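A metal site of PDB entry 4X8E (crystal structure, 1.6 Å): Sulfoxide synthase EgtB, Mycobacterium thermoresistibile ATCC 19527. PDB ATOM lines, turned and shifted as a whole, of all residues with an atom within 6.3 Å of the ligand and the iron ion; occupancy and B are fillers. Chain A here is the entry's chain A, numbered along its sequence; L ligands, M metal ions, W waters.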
ATOM      1  N   TRP A  48      18.339   8.457 -16.462  1.00  0.00           N
ATOM      2  CA  TRP A  48      16.962   8.026 -16.607  1.00  0.00           C
ATOM      3  C   TRP A  48      16.582   7.152 -15.391  1.00  0.00           C
ATOM      4  O   TRP A  48      15.524   7.367 -14.758  1.00  0.00           O
ATOM      5  CB  TRP A  48      16.748   7.264 -17.923  1.00  0.00           C
ATOM      6  CG  TRP A  48      15.283   6.917 -18.148  1.00  0.00           C
ATOM      7  CD1 TRP A  48      14.364   7.648 -18.843  1.00  0.00           C
ATOM      8  CD2 TRP A  48      14.572   5.760 -17.649  1.00  0.00           C
ATOM      9  NE1 TRP A  48      13.145   7.025 -18.819  1.00  0.00           N
ATOM     10  CE2 TRP A  48      13.233   5.894 -18.058  1.00  0.00           C
ATOM     11  CE3 TRP A  48      14.934   4.662 -16.862  1.00  0.00           C
ATOM     12  CZ2 TRP A  48      12.276   4.939 -17.761  1.00  0.00           C
ATOM     13  CZ3 TRP A  48      13.982   3.733 -16.554  1.00  0.00           C
ATOM     14  CH2 TRP A  48      12.670   3.883 -16.985  1.00  0.00           C
ATOM     15  N   HIS A  52      13.704   7.902 -12.598  1.00  0.00           N
ATOM     16  CA  HIS A  52      12.662   6.890 -12.575  1.00  0.00           C
ATOM     17  C   HIS A  52      12.517   6.282 -11.185  1.00  0.00           C
ATOM     18  O   HIS A  52      11.398   6.057 -10.709  1.00  0.00           O
ATOM     19  CB  HIS A  52      12.991   5.777 -13.578  1.00  0.00           C
ATOM     20  CG  HIS A  52      12.127   4.551 -13.446  1.00  0.00           C
ATOM     21  ND1 HIS A  52      10.897   4.422 -14.068  1.00  0.00           N
ATOM     22  CD2 HIS A  52      12.343   3.399 -12.802  1.00  0.00           C
ATOM     23  CE1 HIS A  52      10.401   3.229 -13.797  1.00  0.00           C
ATOM     24  NE2 HIS A  52      11.251   2.579 -13.027  1.00  0.00           N
ATOM     25  N   GLN A  56       9.019   6.568  -9.118  1.00  0.00           N
ATOM     26  CA  GLN A  56       8.316   5.387  -8.670  1.00  0.00           C
ATOM     27  C   GLN A  56       8.167   5.412  -7.156  1.00  0.00           C
ATOM     28  O   GLN A  56       7.116   5.060  -6.621  1.00  0.00           O
ATOM     29  CB  GLN A  56       9.054   4.129  -9.130  1.00  0.00           C
ATOM     30  CG  GLN A  56       8.914   3.920 -10.644  1.00  0.00           C
ATOM     31  CD  GLN A  56       7.602   3.304 -11.012  1.00  0.00           C
ATOM     32  OE1 GLN A  56       7.368   2.142 -10.706  1.00  0.00           O
ATOM     33  NE2 GLN A  56       6.720   4.094 -11.602  1.00  0.00           N
ATOM     34  N   ALA A  83       8.397   3.294 -18.431  1.00  0.00           N
ATOM     35  CA  ALA A  83       9.117   2.327 -19.237  1.00  0.00           C
ATOM     36  C   ALA A  83       8.276   1.686 -20.328  1.00  0.00           C
ATOM     37  O   ALA A  83       8.827   1.177 -21.301  1.00  0.00           O
ATOM     38  CB  ALA A  83       9.702   1.248 -18.341  1.00  0.00           C
ATOM     39  N   ARG A  88      13.782   1.338 -24.483  1.00  0.00           N
ATOM     40  CA  ARG A  88      15.101   1.647 -23.939  1.00  0.00           C
ATOM     41  C   ARG A  88      15.969   2.515 -24.826  1.00  0.00           C
ATOM     42  O   ARG A  88      16.536   3.503 -24.352  1.00  0.00           O
ATOM     43  CB  ARG A  88      15.844   0.341 -23.657  1.00  0.00           C
ATOM     44  CG  ARG A  88      15.387  -0.416 -22.419  1.00  0.00           C
ATOM     45  CD  ARG A  88      16.174  -0.001 -21.185  1.00  0.00           C
ATOM     46  NE  ARG A  88      15.793  -0.755 -19.988  1.00  0.00           N
ATOM     47  CZ  ARG A  88      16.412  -1.828 -19.518  1.00  0.00           C
ATOM     48  NH1 ARG A  88      17.454  -2.364 -20.115  1.00  0.00           N
ATOM     49  NH2 ARG A  88      15.951  -2.386 -18.411  1.00  0.00           N
ATOM     50  N   HIS A 135      12.259  -2.384  -5.804  1.00  0.00           N
ATOM     51  CA  HIS A 135      12.299  -1.659  -7.079  1.00  0.00           C
ATOM     52  C   HIS A 135      13.635  -0.901  -7.271  1.00  0.00           C
ATOM     53  O   HIS A 135      14.266  -1.008  -8.324  1.00  0.00           O
ATOM     54  CB  HIS A 135      11.120  -0.653  -7.170  1.00  0.00           C
ATOM     55  CG  HIS A 135      11.103   0.083  -8.472  1.00  0.00           C
ATOM     56  ND1 HIS A 135      11.562   1.379  -8.602  1.00  0.00           N
ATOM     57  CD2 HIS A 135      10.821  -0.339  -9.723  1.00  0.00           C
ATOM     58  CE1 HIS A 135      11.497   1.747  -9.870  1.00  0.00           C
ATOM     59  NE2 HIS A 135      11.052   0.716 -10.590  1.00  0.00           N
ATOM     60  N   GLN A 138      16.562  -3.307  -7.820  1.00  0.00           N
ATOM     61  CA  GLN A 138      16.531  -3.906  -9.140  1.00  0.00           C
ATOM     62  C   GLN A 138      17.027  -2.929 -10.211  1.00  0.00           C
ATOM     63  O   GLN A 138      17.772  -3.338 -11.123  1.00  0.00           O
ATOM     64  CB  GLN A 138      15.126  -4.428  -9.477  1.00  0.00           C
ATOM     65  CG  GLN A 138      14.758  -5.614  -8.574  1.00  0.00           C
ATOM     66  CD  GLN A 138      13.498  -6.298  -9.015  1.00  0.00           C
ATOM     67  OE1 GLN A 138      13.458  -6.900 -10.088  1.00  0.00           O
ATOM     68  NE2 GLN A 138      12.446  -6.221  -8.216  1.00  0.00           N
ATOM     69  N   HIS A 139      16.679  -1.657 -10.104  1.00  0.00           N
ATOM     70  CA  HIS A 139      17.256  -0.680 -11.030  1.00  0.00           C
ATOM     71  C   HIS A 139      18.750  -0.513 -10.783  1.00  0.00           C
ATOM     72  O   HIS A 139      19.508  -0.212 -11.713  1.00  0.00           O
ATOM     73  CB  HIS A 139      16.534   0.652 -10.963  1.00  0.00           C
ATOM     74  CG  HIS A 139      15.277   0.653 -11.778  1.00  0.00           C
ATOM     75  ND1 HIS A 139      15.263   0.995 -13.113  1.00  0.00           N
ATOM     76  CD2 HIS A 139      14.014   0.284 -11.469  1.00  0.00           C
ATOM     77  CE1 HIS A 139      14.024   0.828 -13.589  1.00  0.00           C
ATOM     78  NE2 HIS A 139      13.246   0.420 -12.606  1.00  0.00           N
ATOM     79  N   THR A 142      20.216  -3.057 -12.875  1.00  0.00           N
ATOM     80  CA  THR A 142      20.172  -2.591 -14.254  1.00  0.00           C
ATOM     81  C   THR A 142      21.294  -1.592 -14.550  1.00  0.00           C
ATOM     82  O   THR A 142      21.960  -1.678 -15.590  1.00  0.00           O
ATOM     83  CB  THR A 142      18.798  -1.956 -14.552  1.00  0.00           C
ATOM     84  OG1 THR A 142      17.810  -2.997 -14.379  1.00  0.00           O
ATOM     85  CG2 THR A 142      18.765  -1.413 -15.964  1.00  0.00           C
ATOM     86  N   TYR A 378       1.369  -2.016  -7.481  1.00  0.00           N
ATOM     87  CA  TYR A 378       1.979  -1.856  -8.792  1.00  0.00           C
ATOM     88  C   TYR A 378       1.478  -3.005  -9.676  1.00  0.00           C
ATOM     89  O   TYR A 378       2.146  -4.039  -9.877  1.00  0.00           O
ATOM     90  CB  TYR A 378       3.502  -1.813  -8.632  1.00  0.00           C
ATOM     91  CG  TYR A 378       4.366  -1.596  -9.858  1.00  0.00           C
ATOM     92  CD1 TYR A 378       3.814  -1.462 -11.123  1.00  0.00           C
ATOM     93  CD2 TYR A 378       5.734  -1.514  -9.718  1.00  0.00           C
ATOM     94  CE1 TYR A 378       4.627  -1.288 -12.222  1.00  0.00           C
ATOM     95  CE2 TYR A 378       6.551  -1.325 -10.801  1.00  0.00           C
ATOM     96  CZ  TYR A 378       5.993  -1.212 -12.064  1.00  0.00           C
ATOM     97  OH  TYR A 378       6.809  -1.024 -13.147  1.00  0.00           O
ATOM     98  N   TYR A 381       3.442  -4.591 -12.661  1.00  0.00           N
ATOM     99  CA  TYR A 381       4.784  -5.112 -12.412  1.00  0.00           C
ATOM    100  C   TYR A 381       5.001  -6.499 -13.051  1.00  0.00           C
ATOM    101  O   TYR A 381       6.046  -6.724 -13.679  1.00  0.00           O
ATOM    102  CB  TYR A 381       5.051  -5.202 -10.905  1.00  0.00           C
ATOM    103  CG  TYR A 381       6.412  -5.791 -10.581  1.00  0.00           C
ATOM    104  CD1 TYR A 381       7.581  -5.019 -10.567  1.00  0.00           C
ATOM    105  CD2 TYR A 381       6.542  -7.119 -10.290  1.00  0.00           C
ATOM    106  CE1 TYR A 381       8.811  -5.566 -10.280  1.00  0.00           C
ATOM    107  CE2 TYR A 381       7.763  -7.658  -9.991  1.00  0.00           C
ATOM    108  CZ  TYR A 381       8.889  -6.901 -10.001  1.00  0.00           C
ATOM    109  OH  TYR A 381      10.098  -7.499  -9.738  1.00  0.00           O
ATOM    110  N   PHE A 385       3.669  -9.347 -18.457  1.00  0.00           N
ATOM    111  CA  PHE A 385       4.739 -10.206 -18.925  1.00  0.00           C
ATOM    112  C   PHE A 385       4.404 -11.674 -18.787  1.00  0.00           C
ATOM    113  O   PHE A 385       5.218 -12.532 -19.134  1.00  0.00           O
ATOM    114  CB  PHE A 385       6.038  -9.831 -18.185  1.00  0.00           C
ATOM    115  CG  PHE A 385       6.263  -8.345 -18.183  1.00  0.00           C
ATOM    116  CD1 PHE A 385       6.547  -7.695 -19.371  1.00  0.00           C
ATOM    117  CD2 PHE A 385       6.067  -7.584 -17.033  1.00  0.00           C
ATOM    118  CE1 PHE A 385       6.671  -6.303 -19.410  1.00  0.00           C
ATOM    119  CE2 PHE A 385       6.200  -6.194 -17.072  1.00  0.00           C
ATOM    120  CZ  PHE A 385       6.509  -5.569 -18.266  1.00  0.00           C
ATOM    121  N   PHE A 413      11.632 -15.633  -5.286  1.00  0.00           N
ATOM    122  CA  PHE A 413      11.713 -14.474  -6.170  1.00  0.00           C
ATOM    123  C   PHE A 413      11.839 -14.890  -7.633  1.00  0.00           C
ATOM    124  O   PHE A 413      12.584 -15.813  -7.951  1.00  0.00           O
ATOM    125  CB  PHE A 413      12.909 -13.556  -5.781  1.00  0.00           C
ATOM    126  CG  PHE A 413      12.928 -12.271  -6.541  1.00  0.00           C
ATOM    127  CD1 PHE A 413      13.467 -12.229  -7.823  1.00  0.00           C
ATOM    128  CD2 PHE A 413      12.350 -11.136  -5.994  1.00  0.00           C
ATOM    129  CE1 PHE A 413      13.449 -11.054  -8.566  1.00  0.00           C
ATOM    130  CE2 PHE A 413      12.347  -9.930  -6.712  1.00  0.00           C
ATOM    131  CZ  PHE A 413      12.885  -9.903  -8.011  1.00  0.00           C
ATOM    132  N   ARG A 414      11.100 -14.197  -8.508  1.00  0.00           N
ATOM    133  CA  ARG A 414      11.091 -14.518  -9.923  1.00  0.00           C
ATOM    134  C   ARG A 414      11.574 -13.340 -10.756  1.00  0.00           C
ATOM    135  O   ARG A 414      10.925 -12.301 -10.789  1.00  0.00           O
ATOM    136  CB  ARG A 414       9.690 -14.920 -10.365  1.00  0.00           C
ATOM    137  CG  ARG A 414       9.114 -16.039  -9.493  1.00  0.00           C
ATOM    138  CD  ARG A 414       7.639 -16.302  -9.731  1.00  0.00           C
ATOM    139  NE  ARG A 414       7.382 -17.007 -10.977  1.00  0.00           N
ATOM    140  CZ  ARG A 414       6.180 -17.122 -11.514  1.00  0.00           C
ATOM    141  NH1 ARG A 414       5.128 -16.556 -10.961  1.00  0.00           N
ATOM    142  NH2 ARG A 414       6.028 -17.825 -12.634  1.00  0.00           N
ATOM    143  N   ASN A 415      12.711 -13.493 -11.418  1.00  0.00           N
ATOM    144  CA  ASN A 415      13.153 -12.561 -12.460  1.00  0.00           C
ATOM    145  C   ASN A 415      12.697 -13.133 -13.797  1.00  0.00           C
ATOM    146  O   ASN A 415      12.314 -14.305 -13.868  1.00  0.00           O
ATOM    147  CB  ASN A 415      14.682 -12.419 -12.358  1.00  0.00           C
ATOM    148  CG  ASN A 415      15.301 -11.402 -13.295  1.00  0.00           C
ATOM    149  OD1 ASN A 415      14.634 -10.530 -13.894  1.00  0.00           O
ATOM    150  ND2 ASN A 415      16.637 -11.479 -13.363  1.00  0.00           N
ATOM    151  N   TRP A 416      12.718 -12.332 -14.851  1.00  0.00           N
ATOM    152  CA  TRP A 416      12.384 -12.821 -16.180  1.00  0.00           C
ATOM    153  C   TRP A 416      12.980 -11.884 -17.206  1.00  0.00           C
ATOM    154  O   TRP A 416      13.232 -10.685 -16.951  1.00  0.00           O
ATOM    155  CB  TRP A 416      10.852 -12.920 -16.386  1.00  0.00           C
ATOM    156  CG  TRP A 416      10.147 -11.597 -16.307  1.00  0.00           C
ATOM    157  CD1 TRP A 416       9.887 -10.758 -17.340  1.00  0.00           C
ATOM    158  CD2 TRP A 416       9.612 -10.955 -15.130  1.00  0.00           C
ATOM    159  NE1 TRP A 416       9.253  -9.627 -16.890  1.00  0.00           N
ATOM    160  CE2 TRP A 416       9.056  -9.722 -15.539  1.00  0.00           C
ATOM    161  CE3 TRP A 416       9.548 -11.313 -13.771  1.00  0.00           C
ATOM    162  CZ2 TRP A 416       8.447  -8.826 -14.644  1.00  0.00           C
ATOM    163  CZ3 TRP A 416       8.938 -10.420 -12.867  1.00  0.00           C
ATOM    164  CH2 TRP A 416       8.385  -9.192 -13.320  1.00  0.00           C
ATOM    165  N   ASP A 417      13.232 -12.421 -18.390  1.00  0.00           N
ATOM    166  CA  ASP A 417      13.666 -11.579 -19.479  1.00  0.00           C
ATOM    167  C   ASP A 417      13.422 -12.261 -20.812  1.00  0.00           C
ATOM    168  O   ASP A 417      13.156 -13.457 -20.883  1.00  0.00           O
ATOM    169  CB  ASP A 417      15.160 -11.215 -19.308  1.00  0.00           C
ATOM    170  CG  ASP A 417      15.433  -9.789 -19.711  1.00  0.00           C
ATOM    171  OD1 ASP A 417      14.814  -9.275 -20.689  1.00  0.00           O
ATOM    172  OD2 ASP A 417      16.224  -9.127 -18.988  1.00  0.00           O
HETATM  173  C1  LIG L   1      11.888  -8.077 -12.862  1.00  0.00           C
HETATM  174  C2  LIG L   1      14.066  -7.197 -13.333  1.00  0.00           C
HETATM  175  C3  LIG L   1      12.565  -7.833 -15.063  1.00  0.00           C
HETATM  176  O1  LIG L   1      12.032  -4.591 -15.801  1.00  0.00           O
HETATM  177  O2  LIG L   1      13.909  -4.566 -14.666  1.00  0.00           O
HETATM  178  C4  LIG L   1      11.978  -2.519 -12.322  1.00  0.00           C
HETATM  179  C5  LIG L   1      12.100  -5.137 -12.399  1.00  0.00           C
HETATM  180  N1  LIG L   1      10.107  -3.618 -12.926  1.00  0.00           N
HETATM  181  N2  LIG L   1      10.965  -1.608 -12.584  1.00  0.00           N
HETATM  182  C6  LIG L   1      12.714  -4.962 -14.800  1.00  0.00           C
HETATM  183  C7  LIG L   1      11.414  -3.760 -12.536  1.00  0.00           C
HETATM  184  C8  LIG L   1       9.832  -2.252 -12.944  1.00  0.00           C
HETATM  185  C9  LIG L   1      12.061  -5.834 -13.770  1.00  0.00           C
HETATM  186  N3  LIG L   1      12.646  -7.201 -13.766  1.00  0.00           N
HETATM  187 FE    FE M   1      11.144   0.495 -12.634  1.00  0.00          FE
HETATM  188  O   HOH W   1      11.015   0.287 -14.709  1.00  0.00           O
HETATM  189  O   HOH W   2      12.387  -8.285 -18.347  1.00  0.00           O
HETATM  190  O   HOH W   3       8.190  -5.181 -14.085  1.00  0.00           O
HETATM  191  O   HOH W   4      11.667  -1.928 -16.321  1.00  0.00           O
HETATM  192  O   HOH W   5       8.944   0.738 -12.623  1.00  0.00           O
HETATM  193  O   HOH W   6      13.349  -5.382 -18.240  1.00  0.00           O
HETATM  194  O   HOH W   7       9.520  -5.200 -16.474  1.00  0.00           O
HETATM  195  O   HOH W   8      16.839  -5.539 -12.711  1.00  0.00           O
HETATM  196  O   HOH W   9      15.287  -2.251 -14.804  1.00  0.00           O
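The iron ion is bound by a ring nitrogen (NE2) of His 135, water W1, a ring nitrogen (NE2) of His 139, a nitrogen (N2) of the ligand, a ring nitrogen (NE2) of His 52 and water W5.
Water W5 bridges the side-chain hydroxyl of Tyr 378 (2.8 Å) and the side-chain amide oxygen of Gln 56 (2.9 Å).
Water W9 bridges OG1 of Thr 142 (2.7 Å) and O2 of the ligand (2.7 Å).
Water W3 lies within hydrogen-bond range of O of Tyr 381 and N1 of the ligand.
Water W8 bridges O of Gln 138 (2.9 Å) and OG1 of Thr 142 (3.2 Å).
Merely in contact with the ligand: Gln 138 (3.2 Å), Tyr 378 (3.3 Å), Asn 415 (3.4 Å), Trp 416 (3.5 Å) and Tyr 381 (3.5 Å).
Hydrophobic or aromatic side chains within 4 Å of the ligand: His 135, His 139, Tyr 381 and Trp 416.
Of the 17 residues printed, 7 come within 4 Å of the ligand.
The nearest printed residue that does not touch the ligand is Thr 142 (4.2 Å).
The side-chain amide nitrogen (NE2) of Gln 138 lies within hydrogen-bond range of the side-chain hydroxyl (OH) of Tyr 381.
The backbone carbonyl oxygen of Gln 138 sits at hydrogen-bond distance from the side-chain hydroxyl of Thr 142 (3.3 Å).
Within 4 Å of the iron ion: His 52, His 135 and His 139.
The nearest printed residue that does not touch the iron ion is Gln 56 (4.5 Å).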
